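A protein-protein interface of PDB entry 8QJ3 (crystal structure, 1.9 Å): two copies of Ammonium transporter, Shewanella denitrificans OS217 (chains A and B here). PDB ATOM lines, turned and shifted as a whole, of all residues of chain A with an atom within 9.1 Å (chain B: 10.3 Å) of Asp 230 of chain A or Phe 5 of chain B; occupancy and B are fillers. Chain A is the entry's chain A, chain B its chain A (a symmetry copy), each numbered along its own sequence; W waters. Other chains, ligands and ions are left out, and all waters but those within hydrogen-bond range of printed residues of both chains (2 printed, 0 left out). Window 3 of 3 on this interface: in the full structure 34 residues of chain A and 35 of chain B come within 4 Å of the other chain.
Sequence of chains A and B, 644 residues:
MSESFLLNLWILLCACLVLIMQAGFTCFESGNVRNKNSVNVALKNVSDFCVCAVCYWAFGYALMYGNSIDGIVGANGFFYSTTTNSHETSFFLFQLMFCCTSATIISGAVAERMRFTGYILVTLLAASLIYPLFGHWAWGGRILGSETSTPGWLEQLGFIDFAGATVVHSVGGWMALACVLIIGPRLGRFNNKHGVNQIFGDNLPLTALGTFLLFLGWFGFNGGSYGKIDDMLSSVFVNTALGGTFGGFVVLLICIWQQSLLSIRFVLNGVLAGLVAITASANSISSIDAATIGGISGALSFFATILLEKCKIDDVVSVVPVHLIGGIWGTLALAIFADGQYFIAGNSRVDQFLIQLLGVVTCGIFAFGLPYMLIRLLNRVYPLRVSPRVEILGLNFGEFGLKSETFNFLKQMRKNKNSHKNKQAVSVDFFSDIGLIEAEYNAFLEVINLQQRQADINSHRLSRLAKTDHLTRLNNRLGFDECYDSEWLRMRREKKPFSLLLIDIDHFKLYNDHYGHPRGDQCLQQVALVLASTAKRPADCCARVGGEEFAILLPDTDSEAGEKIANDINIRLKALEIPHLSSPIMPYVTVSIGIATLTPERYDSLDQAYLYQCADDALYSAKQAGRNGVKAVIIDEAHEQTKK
Water W2 lies within hydrogen-bond range of the side-chain amide oxygen of Asn 8 of chain B (2.5 Å), the side-chain hydroxyl of Ser 234 of chain A (2.8 Å), the backbone NH of Ser 90 of chain B (3.0 Å), the backbone carbonyl oxygen of Ser 86 of chain B (3.1 Å) and the backbone NH of Thr 89 of chain B (3.4 Å).
Positions printed for both chains: 3, 6, 7, 10 and 229.
Printed residues of chain B that touch a printed residue of chain A: Phe 5, Leu 9, Leu 12, Leu 13, Thr 89 and Ser 90. Hydrophobic or aromatic side chains of chain B within 4 Å of the printed part of chain A: Phe 5, Leu 9, Leu 12 and Leu 13. Along chain B the printed residues that touch a printed residue of chain A span positions 5 to 90. Hydrophobic or aromatic side chains of chain A within 4 Å of the printed part of chain B: Leu 6, Trp 10, Ile 229 and Leu 233. Along chain A the printed residues that touch a printed residue of chain B span positions 6 to 235.
CD1 of Leu 9 of chain B touches CD1 of Leu 6 of chain A, 3.6 Å away. Leu 9 of chain B touches Trp 10 of chain A (CD2 to CZ3, 3.7 Å). Phe 5 of chain B touches Ile 229 of chain A. CA of Asp 230 of chain A touches CZ of Phe 5 of chain B (3.8 Å). Ser 234 of chain A touches Leu 12 of chain B. OG of Ser 234 of chain A touches CB of Thr 89 of chain B, at 3.2 Å. Ser 234 of chain A touches Ser 90 of chain B.
Asp 230 of chain A touches just one residue of chain B: Phe 5 (3.8 Å). No residue of chain B comes within 4 Å of Asp 231 of chain A. Of the printed residues of chain B, Ser 235 of chain A touches Thr 89. No residue of chain A comes within 4 Å of Ser 2 of chain B. Ser 4 of chain B touches none of the printed residues of chain A. Leu 6 of chain B touches none of the printed residues of chain A. Of the printed residues of chain A, Leu 9 of chain B touches Leu 6, Trp 10, Ile 229 and Leu 233. Printed residues of chain A within 4 Å of Leu 12 of chain B: Ser 234 (3.9 Å). The nearest printed residue of chain A that does not touch Phe 5 of chain B is Asp 231 of chain A (4.1 Å).
The side-chain carboxylate of Asp 230 of chain A lies within hydrogen-bond range of the side-chain hydroxyl of Tyr 226 of chain A, at 2.6 Å. The side-chain amide oxygen (OD1) of Asn 8 of chain B is in hydrogen-bond range of the side-chain hydroxyl (OG) of Ser 90 of chain B (2.7 Å).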
ATOM      1  N   GLU A   3      -4.532 -17.001  29.453  1.00  0.00           N
ATOM      2  CA  GLU A   3      -4.831 -17.279  28.056  1.00  0.00           C
ATOM      3  C   GLU A   3      -4.072 -16.302  27.158  1.00  0.00           C
ATOM      4  O   GLU A   3      -3.564 -16.682  26.100  1.00  0.00           O
ATOM      5  CB  GLU A   3      -6.342 -17.193  27.811  1.00  0.00           C
ATOM      6  CG  GLU A   3      -6.809 -17.927  26.550  1.00  0.00           C
ATOM      7  CD  GLU A   3      -7.010 -17.109  25.281  1.00  0.00           C
ATOM      8  OE1 GLU A   3      -7.783 -16.134  25.337  1.00  0.00           O
ATOM      9  OE2 GLU A   3      -6.435 -17.477  24.228  1.00  0.00           O
ATOM     10  N   LEU A   6      -0.306 -16.537  24.738  1.00  0.00           N
ATOM     11  CA  LEU A   6       0.090 -16.963  23.404  1.00  0.00           C
ATOM     12  C   LEU A   6      -0.026 -15.755  22.463  1.00  0.00           C
ATOM     13  O   LEU A   6       0.868 -15.529  21.664  1.00  0.00           O
ATOM     14  CB  LEU A   6      -0.738 -18.163  22.916  1.00  0.00           C
ATOM     15  CG  LEU A   6      -0.377 -18.671  21.511  1.00  0.00           C
ATOM     16  CD1 LEU A   6       1.092 -19.043  21.417  1.00  0.00           C
ATOM     17  CD2 LEU A   6      -1.213 -19.876  21.100  1.00  0.00           C
ATOM     18  N   LEU A   7      -1.141 -14.999  22.519  1.00  0.00           N
ATOM     19  CA  LEU A   7      -1.327 -13.939  21.532  1.00  0.00           C
ATOM     20  C   LEU A   7      -0.247 -12.880  21.748  1.00  0.00           C
ATOM     21  O   LEU A   7       0.316 -12.388  20.779  1.00  0.00           O
ATOM     22  CB  LEU A   7      -2.733 -13.350  21.585  1.00  0.00           C
ATOM     23  CG  LEU A   7      -3.050 -12.177  20.639  1.00  0.00           C
ATOM     24  CD1 LEU A   7      -2.822 -12.495  19.178  1.00  0.00           C
ATOM     25  CD2 LEU A   7      -4.522 -11.768  20.806  1.00  0.00           C
ATOM     26  N   TRP A  10       2.957 -13.983  20.190  1.00  0.00           N
ATOM     27  CA  TRP A  10       2.808 -13.937  18.753  1.00  0.00           C
ATOM     28  C   TRP A  10       3.049 -12.524  18.214  1.00  0.00           C
ATOM     29  O   TRP A  10       3.805 -12.323  17.270  1.00  0.00           O
ATOM     30  CB  TRP A  10       1.432 -14.452  18.349  1.00  0.00           C
ATOM     31  CG  TRP A  10       1.189 -14.414  16.859  1.00  0.00           C
ATOM     32  CD1 TRP A  10       0.308 -13.629  16.187  1.00  0.00           C
ATOM     33  CD2 TRP A  10       1.821 -15.228  15.849  1.00  0.00           C
ATOM     34  NE1 TRP A  10       0.381 -13.828  14.838  1.00  0.00           N
ATOM     35  CE2 TRP A  10       1.292 -14.823  14.599  1.00  0.00           C
ATOM     36  CE3 TRP A  10       2.750 -16.255  15.885  1.00  0.00           C
ATOM     37  CZ2 TRP A  10       1.662 -15.425  13.393  1.00  0.00           C
ATOM     38  CZ3 TRP A  10       3.110 -16.853  14.695  1.00  0.00           C
ATOM     39  CH2 TRP A  10       2.561 -16.452  13.479  1.00  0.00           C
ATOM     40  N   TYR A 226      -3.504  -9.833  12.541  1.00  0.00           N
ATOM     41  CA  TYR A 226      -4.615 -10.759  12.471  1.00  0.00           C
ATOM     42  C   TYR A 226      -5.572 -10.612  13.649  1.00  0.00           C
ATOM     43  O   TYR A 226      -6.741 -10.963  13.504  1.00  0.00           O
ATOM     44  CB  TYR A 226      -4.104 -12.189  12.417  1.00  0.00           C
ATOM     45  CG  TYR A 226      -5.125 -13.228  11.956  1.00  0.00           C
ATOM     46  CD1 TYR A 226      -5.622 -13.229  10.670  1.00  0.00           C
ATOM     47  CD2 TYR A 226      -5.590 -14.211  12.818  1.00  0.00           C
ATOM     48  CE1 TYR A 226      -6.564 -14.152  10.246  1.00  0.00           C
ATOM     49  CE2 TYR A 226      -6.492 -15.182  12.399  1.00  0.00           C
ATOM     50  CZ  TYR A 226      -6.950 -15.176  11.101  1.00  0.00           C
ATOM     51  OH  TYR A 226      -7.850 -16.112  10.719  1.00  0.00           O
ATOM     52  N   GLY A 227      -5.094 -10.117  14.790  1.00  0.00           N
ATOM     53  CA  GLY A 227      -5.979  -9.726  15.865  1.00  0.00           C
ATOM     54  C   GLY A 227      -6.377 -10.878  16.771  1.00  0.00           C
ATOM     55  O   GLY A 227      -7.253 -10.755  17.611  1.00  0.00           O
ATOM     56  N   LYS A 228      -5.748 -12.016  16.627  1.00  0.00           N
ATOM     57  CA  LYS A 228      -6.263 -13.117  17.405  1.00  0.00           C
ATOM     58  C   LYS A 228      -5.517 -14.316  16.899  1.00  0.00           C
ATOM     59  O   LYS A 228      -4.607 -14.130  16.049  1.00  0.00           O
ATOM     60  CB  LYS A 228      -7.698 -13.492  17.096  1.00  0.00           C
ATOM     61  CG  LYS A 228      -7.946 -14.007  15.688  1.00  0.00           C
ATOM     62  CD  LYS A 228      -8.896 -13.063  14.963  1.00  0.00           C
ATOM     63  CE  LYS A 228      -9.588 -13.669  13.768  1.00  0.00           C
ATOM     64  NZ  LYS A 228      -9.070 -13.048  12.523  1.00  0.00           N
ATOM     65  N   ILE A 229      -5.920 -15.493  17.377  1.00  0.00           N
ATOM     66  CA  ILE A 229      -5.509 -16.699  16.697  1.00  0.00           C
ATOM     67  C   ILE A 229      -6.749 -17.546  16.470  1.00  0.00           C
ATOM     68  O   ILE A 229      -7.615 -17.613  17.329  1.00  0.00           O
ATOM     69  CB  ILE A 229      -4.418 -17.443  17.472  1.00  0.00           C
ATOM     70  CG1 ILE A 229      -3.216 -16.535  17.759  1.00  0.00           C
ATOM     71  CG2 ILE A 229      -4.037 -18.694  16.694  1.00  0.00           C
ATOM     72  CD1 ILE A 229      -2.383 -16.978  18.940  1.00  0.00           C
ATOM     73  N   ASP A 230      -6.873 -18.055  15.245  1.00  0.00           N
ATOM     74  CA  ASP A 230      -7.799 -19.120  14.930  1.00  0.00           C
ATOM     75  C   ASP A 230      -7.113 -19.989  13.877  1.00  0.00           C
ATOM     76  O   ASP A 230      -5.952 -19.733  13.507  1.00  0.00           O
ATOM     77  CB  ASP A 230      -9.164 -18.557  14.543  1.00  0.00           C
ATOM     78  CG  ASP A 230      -9.111 -17.778  13.245  1.00  0.00           C
ATOM     79  OD1 ASP A 230      -8.175 -18.047  12.424  1.00  0.00           O
ATOM     80  OD2 ASP A 230      -9.980 -16.911  13.064  1.00  0.00           O
ATOM     81  N   ASP A 231      -7.860 -20.975  13.373  1.00  0.00           N
ATOM     82  CA  ASP A 231      -7.286 -21.973  12.486  1.00  0.00           C
ATOM     83  C   ASP A 231      -7.140 -21.421  11.067  1.00  0.00           C
ATOM     84  O   ASP A 231      -6.680 -22.162  10.212  1.00  0.00           O
ATOM     85  CB  ASP A 231      -8.124 -23.270  12.449  1.00  0.00           C
ATOM     86  CG  ASP A 231      -9.583 -23.123  12.002  1.00  0.00           C
ATOM     87  OD1 ASP A 231      -9.992 -21.994  11.625  1.00  0.00           O
ATOM     88  OD2 ASP A 231     -10.338 -24.157  12.050  1.00  0.00           O
ATOM     89  N   MET A 232      -7.568 -20.182  10.785  1.00  0.00           N
ATOM     90  CA  MET A 232      -7.330 -19.611   9.470  1.00  0.00           C
ATOM     91  C   MET A 232      -6.070 -18.719   9.405  1.00  0.00           C
ATOM     92  O   MET A 232      -5.766 -18.165   8.341  1.00  0.00           O
ATOM     93  CB  MET A 232      -8.572 -18.851   8.996  1.00  0.00           C
ATOM     94  CG  MET A 232      -9.700 -19.795   8.507  1.00  0.00           C
ATOM     95  SD  MET A 232      -9.258 -20.790   7.027  1.00  0.00           S
ATOM     96  CE  MET A 232      -9.410 -19.497   5.788  1.00  0.00           C
ATOM     97  N   LEU A 233      -5.292 -18.607  10.494  1.00  0.00           N
ATOM     98  CA  LEU A 233      -4.112 -17.732  10.471  1.00  0.00           C
ATOM     99  C   LEU A 233      -3.134 -18.189   9.399  1.00  0.00           C
ATOM    100  O   LEU A 233      -2.569 -17.364   8.702  1.00  0.00           O
ATOM    101  CB  LEU A 233      -3.482 -17.712  11.861  1.00  0.00           C
ATOM    102  CG  LEU A 233      -2.212 -16.858  12.082  1.00  0.00           C
ATOM    103  CD1 LEU A 233      -2.353 -15.448  11.562  1.00  0.00           C
ATOM    104  CD2 LEU A 233      -1.878 -16.776  13.560  1.00  0.00           C
ATOM    105  N   SER A 234      -2.942 -19.514   9.224  1.00  0.00           N
ATOM    106  CA  SER A 234      -1.947 -19.985   8.286  1.00  0.00           C
ATOM    107  C   SER A 234      -2.283 -19.578   6.846  1.00  0.00           C
ATOM    108  O   SER A 234      -1.375 -19.463   6.031  1.00  0.00           O
ATOM    109  CB  SER A 234      -1.692 -21.486   8.438  1.00  0.00           C
ATOM    110  OG  SER A 234      -2.866 -22.199   8.116  1.00  0.00           O
ATOM    111  N   SER A 235      -3.571 -19.306   6.554  1.00  0.00           N
ATOM    112  CA  SER A 235      -3.993 -18.883   5.227  1.00  0.00           C
ATOM    113  C   SER A 235      -3.521 -17.458   4.902  1.00  0.00           C
ATOM    114  O   SER A 235      -3.258 -17.127   3.758  1.00  0.00           O
ATOM    115  CB  SER A 235      -5.495 -19.044   5.076  1.00  0.00           C
ATOM    116  OG  SER A 235      -5.847 -20.408   5.161  1.00  0.00           O
ATOM    117  N   VAL A 236      -3.343 -16.618   5.911  1.00  0.00           N
ATOM    118  CA  VAL A 236      -2.746 -15.310   5.713  1.00  0.00           C
ATOM    119  C   VAL A 236      -1.283 -15.455   5.251  1.00  0.00           C
ATOM    120  O   VAL A 236      -0.858 -14.787   4.331  1.00  0.00           O
ATOM    121  CB  VAL A 236      -2.828 -14.497   7.010  1.00  0.00           C
ATOM    122  CG1 VAL A 236      -1.876 -13.288   6.979  1.00  0.00           C
ATOM    123  CG2 VAL A 236      -4.268 -14.112   7.342  1.00  0.00           C
ATOM    124  N   ASN A 283      -6.359 -11.804   4.726  1.00  0.00           N
ATOM    125  CA  ASN A 283      -7.230 -12.605   5.577  1.00  0.00           C
ATOM    126  C   ASN A 283      -8.576 -12.973   4.918  1.00  0.00           C
ATOM    127  O   ASN A 283      -9.335 -13.740   5.503  1.00  0.00           O
ATOM    128  CB  ASN A 283      -7.477 -11.856   6.883  1.00  0.00           C
ATOM    129  CG  ASN A 283      -8.282 -10.599   6.644  1.00  0.00           C
ATOM    130  OD1 ASN A 283      -7.993  -9.869   5.705  1.00  0.00           O
ATOM    131  ND2 ASN A 283      -9.305 -10.362   7.453  1.00  0.00           N
ATOM    132  N   GLN A 341     -18.404 -12.081   3.285  1.00  0.00           N
ATOM    133  CA  GLN A 341     -18.697 -12.190   4.706  1.00  0.00           C
ATOM    134  C   GLN A 341     -17.807 -11.239   5.511  1.00  0.00           C
ATOM    135  O   GLN A 341     -18.127 -10.961   6.663  1.00  0.00           O
ATOM    136  CB  GLN A 341     -18.563 -13.655   5.117  1.00  0.00           C
ATOM    137  CG  GLN A 341     -18.223 -13.885   6.589  1.00  0.00           C
ATOM    138  CD  GLN A 341     -17.143 -14.911   6.878  1.00  0.00           C
ATOM    139  OE1 GLN A 341     -16.579 -15.569   5.994  1.00  0.00           O
ATOM    140  NE2 GLN A 341     -16.823 -15.028   8.159  1.00  0.00           N
ATOM    141  N   TYR A 342     -16.677 -10.753   4.938  1.00  0.00           N
ATOM    142  CA  TYR A 342     -15.809  -9.843   5.666  1.00  0.00           C
ATOM    143  C   TYR A 342     -16.276  -8.404   5.551  1.00  0.00           C
ATOM    144  O   TYR A 342     -15.627  -7.528   6.126  1.00  0.00           O
ATOM    145  CB  TYR A 342     -14.356  -9.922   5.163  1.00  0.00           C
ATOM    146  CG  TYR A 342     -13.708 -11.225   5.595  1.00  0.00           C
ATOM    147  CD1 TYR A 342     -13.889 -12.395   4.866  1.00  0.00           C
ATOM    148  CD2 TYR A 342     -12.969 -11.289   6.768  1.00  0.00           C
ATOM    149  CE1 TYR A 342     -13.345 -13.599   5.292  1.00  0.00           C
ATOM    150  CE2 TYR A 342     -12.408 -12.481   7.200  1.00  0.00           C
ATOM    151  CZ  TYR A 342     -12.618 -13.643   6.471  1.00  0.00           C
ATOM    152  OH  TYR A 342     -12.058 -14.817   6.879  1.00  0.00           O
ATOM    153  N   SER B   2      -8.238 -23.820  21.255  1.00  0.00           N
ATOM    154  CA  SER B   2      -8.030 -24.983  20.342  1.00  0.00           C
ATOM    155  C   SER B   2      -6.557 -25.412  20.401  1.00  0.00           C
ATOM    156  O   SER B   2      -5.668 -24.572  20.458  1.00  0.00           O
ATOM    157  CB  SER B   2      -8.531 -24.643  18.940  1.00  0.00           C
ATOM    158  OG  SER B   2      -8.073 -25.558  17.956  1.00  0.00           O
ATOM    159  N   GLU B   3      -6.309 -26.729  20.449  1.00  0.00           N
ATOM    160  CA  GLU B   3      -4.994 -27.266  20.765  1.00  0.00           C
ATOM    161  C   GLU B   3      -4.029 -26.989  19.613  1.00  0.00           C
ATOM    162  O   GLU B   3      -2.860 -26.663  19.834  1.00  0.00           O
ATOM    163  CB  GLU B   3      -5.092 -28.768  21.053  1.00  0.00           C
ATOM    164  CG  GLU B   3      -3.912 -29.325  21.856  1.00  0.00           C
ATOM    165  CD  GLU B   3      -2.782 -30.001  21.088  1.00  0.00           C
ATOM    166  OE1 GLU B   3      -3.079 -30.949  20.338  1.00  0.00           O
ATOM    167  OE2 GLU B   3      -1.604 -29.614  21.281  1.00  0.00           O
ATOM    168  N   SER B   4      -4.574 -27.058  18.391  1.00  0.00           N
ATOM    169  CA  SER B   4      -3.802 -27.066  17.163  1.00  0.00           C
ATOM    170  C   SER B   4      -3.112 -25.712  16.926  1.00  0.00           C
ATOM    171  O   SER B   4      -2.306 -25.607  15.991  1.00  0.00           O
ATOM    172  CB  SER B   4      -4.687 -27.518  15.979  1.00  0.00           C
ATOM    173  OG  SER B   4      -5.293 -26.422  15.310  1.00  0.00           O
ATOM    174  N   PHE B   5      -3.381 -24.701  17.785  1.00  0.00           N
ATOM    175  CA  PHE B   5      -2.830 -23.373  17.540  1.00  0.00           C
ATOM    176  C   PHE B   5      -1.324 -23.379  17.741  1.00  0.00           C
ATOM    177  O   PHE B   5      -0.617 -22.841  16.895  1.00  0.00           O
ATOM    178  CB  PHE B   5      -3.387 -22.264  18.426  1.00  0.00           C
ATOM    179  CG  PHE B   5      -4.842 -21.927  18.239  1.00  0.00           C
ATOM    180  CD1 PHE B   5      -5.590 -22.503  17.218  1.00  0.00           C
ATOM    181  CD2 PHE B   5      -5.477 -21.087  19.159  1.00  0.00           C
ATOM    182  CE1 PHE B   5      -6.950 -22.236  17.117  1.00  0.00           C
ATOM    183  CE2 PHE B   5      -6.835 -20.794  19.030  1.00  0.00           C
ATOM    184  CZ  PHE B   5      -7.566 -21.373  18.010  1.00  0.00           C
ATOM    185  N   LEU B   6      -0.835 -23.935  18.857  1.00  0.00           N
ATOM    186  CA  LEU B   6       0.582 -23.767  19.145  1.00  0.00           C
ATOM    187  C   LEU B   6       1.380 -24.379  17.987  1.00  0.00           C
ATOM    188  O   LEU B   6       2.336 -23.773  17.530  1.00  0.00           O
ATOM    189  CB  LEU B   6       0.966 -24.375  20.504  1.00  0.00           C
ATOM    190  CG  LEU B   6       2.451 -24.237  20.879  1.00  0.00           C
ATOM    191  CD1 LEU B   6       2.890 -22.784  20.873  1.00  0.00           C
ATOM    192  CD2 LEU B   6       2.759 -24.834  22.246  1.00  0.00           C
ATOM    193  N   LEU B   7       1.026 -25.599  17.533  1.00  0.00           N
ATOM    194  CA  LEU B   7       1.865 -26.253  16.533  1.00  0.00           C
ATOM    195  C   LEU B   7       1.811 -25.436  15.243  1.00  0.00           C
ATOM    196  O   LEU B   7       2.839 -25.244  14.608  1.00  0.00           O
ATOM    197  CB  LEU B   7       1.463 -27.707  16.313  1.00  0.00           C
ATOM    198  CG  LEU B   7       2.225 -28.502  15.237  1.00  0.00           C
ATOM    199  CD1 LEU B   7       3.721 -28.548  15.460  1.00  0.00           C
ATOM    200  CD2 LEU B   7       1.711 -29.951  15.211  1.00  0.00           C
ATOM    201  N   ASN B   8       0.621 -24.951  14.842  1.00  0.00           N
ATOM    202  CA  ASN B   8       0.556 -24.126  13.641  1.00  0.00           C
ATOM    203  C   ASN B   8       1.471 -22.914  13.775  1.00  0.00           C
ATOM    204  O   ASN B   8       2.138 -22.591  12.813  1.00  0.00           O
ATOM    205  CB  ASN B   8      -0.851 -23.652  13.260  1.00  0.00           C
ATOM    206  CG  ASN B   8      -1.600 -24.688  12.442  1.00  0.00           C
ATOM    207  OD1 ASN B   8      -1.322 -24.941  11.267  1.00  0.00           O
ATOM    208  ND2 ASN B   8      -2.614 -25.267  13.049  1.00  0.00           N
ATOM    209  N   LEU B   9       1.429 -22.192  14.907  1.00  0.00           N
ATOM    210  CA  LEU B   9       2.241 -20.986  15.032  1.00  0.00           C
ATOM    211  C   LEU B   9       3.719 -21.357  14.916  1.00  0.00           C
ATOM    212  O   LEU B   9       4.438 -20.598  14.297  1.00  0.00           O
ATOM    213  CB  LEU B   9       2.001 -20.250  16.343  1.00  0.00           C
ATOM    214  CG  LEU B   9       0.596 -19.660  16.564  1.00  0.00           C
ATOM    215  CD1 LEU B   9       0.574 -18.795  17.821  1.00  0.00           C
ATOM    216  CD2 LEU B   9       0.092 -18.864  15.403  1.00  0.00           C
ATOM    217  N   TRP B  10       4.109 -22.508  15.485  1.00  0.00           N
ATOM    218  CA  TRP B  10       5.471 -22.989  15.450  1.00  0.00           C
ATOM    219  C   TRP B  10       5.941 -23.222  14.010  1.00  0.00           C
ATOM    220  O   TRP B  10       7.010 -22.774  13.609  1.00  0.00           O
ATOM    221  CB  TRP B  10       5.603 -24.259  16.282  1.00  0.00           C
ATOM    222  CG  TRP B  10       6.997 -24.840  16.276  1.00  0.00           C
ATOM    223  CD1 TRP B  10       7.399 -26.012  15.722  1.00  0.00           C
ATOM    224  CD2 TRP B  10       8.179 -24.283  16.888  1.00  0.00           C
ATOM    225  NE1 TRP B  10       8.743 -26.206  15.871  1.00  0.00           N
ATOM    226  CE2 TRP B  10       9.249 -25.165  16.603  1.00  0.00           C
ATOM    227  CE3 TRP B  10       8.424 -23.153  17.653  1.00  0.00           C
ATOM    228  CZ2 TRP B  10      10.549 -24.950  17.070  1.00  0.00           C
ATOM    229  CZ3 TRP B  10       9.705 -22.946  18.119  1.00  0.00           C
ATOM    230  CH2 TRP B  10      10.739 -23.839  17.843  1.00  0.00           C
ATOM    231  N   ILE B  11       5.140 -23.971  13.256  1.00  0.00           N
ATOM    232  CA  ILE B  11       5.430 -24.250  11.860  1.00  0.00           C
ATOM    233  C   ILE B  11       5.575 -22.930  11.060  1.00  0.00           C
ATOM    234  O   ILE B  11       6.490 -22.841  10.233  1.00  0.00           O
ATOM    235  CB  ILE B  11       4.355 -25.189  11.240  1.00  0.00           C
ATOM    236  CG1 ILE B  11       4.239 -26.528  11.964  1.00  0.00           C
ATOM    237  CG2 ILE B  11       4.611 -25.419   9.761  1.00  0.00           C
ATOM    238  CD1 ILE B  11       5.524 -27.267  12.060  1.00  0.00           C
ATOM    239  N   LEU B  12       4.645 -21.969  11.248  1.00  0.00           N
ATOM    240  CA  LEU B  12       4.693 -20.731  10.499  1.00  0.00           C
ATOM    241  C   LEU B  12       5.998 -19.964  10.783  1.00  0.00           C
ATOM    242  O   LEU B  12       6.649 -19.486   9.850  1.00  0.00           O
ATOM    243  CB  LEU B  12       3.458 -19.891  10.803  1.00  0.00           C
ATOM    244  CG  LEU B  12       2.146 -20.480  10.311  1.00  0.00           C
ATOM    245  CD1 LEU B  12       1.017 -19.630  10.867  1.00  0.00           C
ATOM    246  CD2 LEU B  12       2.112 -20.579   8.796  1.00  0.00           C
ATOM    247  N   LEU B  13       6.402 -19.929  12.060  1.00  0.00           N
ATOM    248  CA  LEU B  13       7.633 -19.246  12.436  1.00  0.00           C
ATOM    249  C   LEU B  13       8.837 -19.993  11.875  1.00  0.00           C
ATOM    250  O   LEU B  13       9.753 -19.368  11.382  1.00  0.00           O
ATOM    251  CB  LEU B  13       7.661 -19.144  13.952  1.00  0.00           C
ATOM    252  CG  LEU B  13       6.705 -18.110  14.533  1.00  0.00           C
ATOM    253  CD1 LEU B  13       6.570 -18.278  16.028  1.00  0.00           C
ATOM    254  CD2 LEU B  13       7.118 -16.727  14.204  1.00  0.00           C
ATOM    255  N   SER B  86      -6.420 -29.191   9.930  1.00  0.00           N
ATOM    256  CA  SER B  86      -6.149 -27.868  10.442  1.00  0.00           C
ATOM    257  C   SER B  86      -4.632 -27.590  10.553  1.00  0.00           C
ATOM    258  O   SER B  86      -4.264 -26.521  10.978  1.00  0.00           O
ATOM    259  CB  SER B  86      -6.834 -27.679  11.751  1.00  0.00           C
ATOM    260  OG  SER B  86      -6.135 -28.412  12.716  1.00  0.00           O
ATOM    261  N   HIS B  87      -3.771 -28.560  10.254  1.00  0.00           N
ATOM    262  CA  HIS B  87      -2.332 -28.355  10.195  1.00  0.00           C
ATOM    263  C   HIS B  87      -1.806 -28.323   8.764  1.00  0.00           C
ATOM    264  O   HIS B  87      -0.625 -28.039   8.560  1.00  0.00           O
ATOM    265  CB  HIS B  87      -1.605 -29.457  10.967  1.00  0.00           C
ATOM    266  CG  HIS B  87      -1.913 -29.426  12.422  1.00  0.00           C
ATOM    267  ND1 HIS B  87      -2.878 -30.235  12.997  1.00  0.00           N
ATOM    268  CD2 HIS B  87      -1.465 -28.630  13.397  1.00  0.00           C
ATOM    269  CE1 HIS B  87      -2.938 -29.991  14.308  1.00  0.00           C
ATOM    270  NE2 HIS B  87      -2.109 -28.991  14.576  1.00  0.00           N
ATOM    271  N   THR B  89      -2.257 -26.340   6.057  1.00  0.00           N
ATOM    272  CA  THR B  89      -1.866 -25.131   5.376  1.00  0.00           C
ATOM    273  C   THR B  89      -0.476 -24.675   5.846  1.00  0.00           C
ATOM    274  O   THR B  89       0.319 -24.220   5.021  1.00  0.00           O
ATOM    275  CB  THR B  89      -2.975 -24.089   5.516  1.00  0.00           C
ATOM    276  OG1 THR B  89      -4.094 -24.701   4.877  1.00  0.00           O
ATOM    277  CG2 THR B  89      -2.662 -22.802   4.849  1.00  0.00           C
ATOM    278  N   SER B  90      -0.245 -24.696   7.154  1.00  0.00           N
ATOM    279  CA  SER B  90       1.058 -24.376   7.685  1.00  0.00           C
ATOM    280  C   SER B  90       2.085 -25.307   7.057  1.00  0.00           C
ATOM    281  O   SER B  90       3.169 -24.903   6.705  1.00  0.00           O
ATOM    282  CB  SER B  90       1.048 -24.531   9.213  1.00  0.00           C
ATOM    283  OG  SER B  90       0.346 -23.398   9.726  1.00  0.00           O
ATOM    284  N   LEU B 144       1.670 -33.606   7.989  1.00  0.00           N
ATOM    285  CA  LEU B 144       1.352 -33.162   9.332  1.00  0.00           C
ATOM    286  C   LEU B 144      -0.164 -33.196   9.552  1.00  0.00           C
ATOM    287  O   LEU B 144      -0.917 -32.588   8.806  1.00  0.00           O
ATOM    288  CB  LEU B 144       1.871 -31.733   9.537  1.00  0.00           C
ATOM    289  CG  LEU B 144       1.799 -31.218  10.972  1.00  0.00           C
ATOM    290  CD1 LEU B 144       2.649 -32.079  11.897  1.00  0.00           C
ATOM    291  CD2 LEU B 144       2.248 -29.785  11.043  1.00  0.00           C
ATOM    292  N   ILE B 229       5.024 -31.174  19.098  1.00  0.00           N
ATOM    293  CA  ILE B 229       5.867 -30.656  20.151  1.00  0.00           C
ATOM    294  C   ILE B 229       5.881 -31.677  21.275  1.00  0.00           C
ATOM    295  O   ILE B 229       4.861 -32.280  21.572  1.00  0.00           O
ATOM    296  CB  ILE B 229       5.406 -29.271  20.616  1.00  0.00           C
ATOM    297  CG1 ILE B 229       5.321 -28.287  19.443  1.00  0.00           C
ATOM    298  CG2 ILE B 229       6.341 -28.793  21.717  1.00  0.00           C
ATOM    299  CD1 ILE B 229       4.387 -27.123  19.688  1.00  0.00           C
HETATM  300  O   HOH W   1      -5.044 -23.960  11.143  1.00  0.00           O
HETATM  301  O   HOH W   2      -2.541 -24.789   9.097  1.00  0.00           O
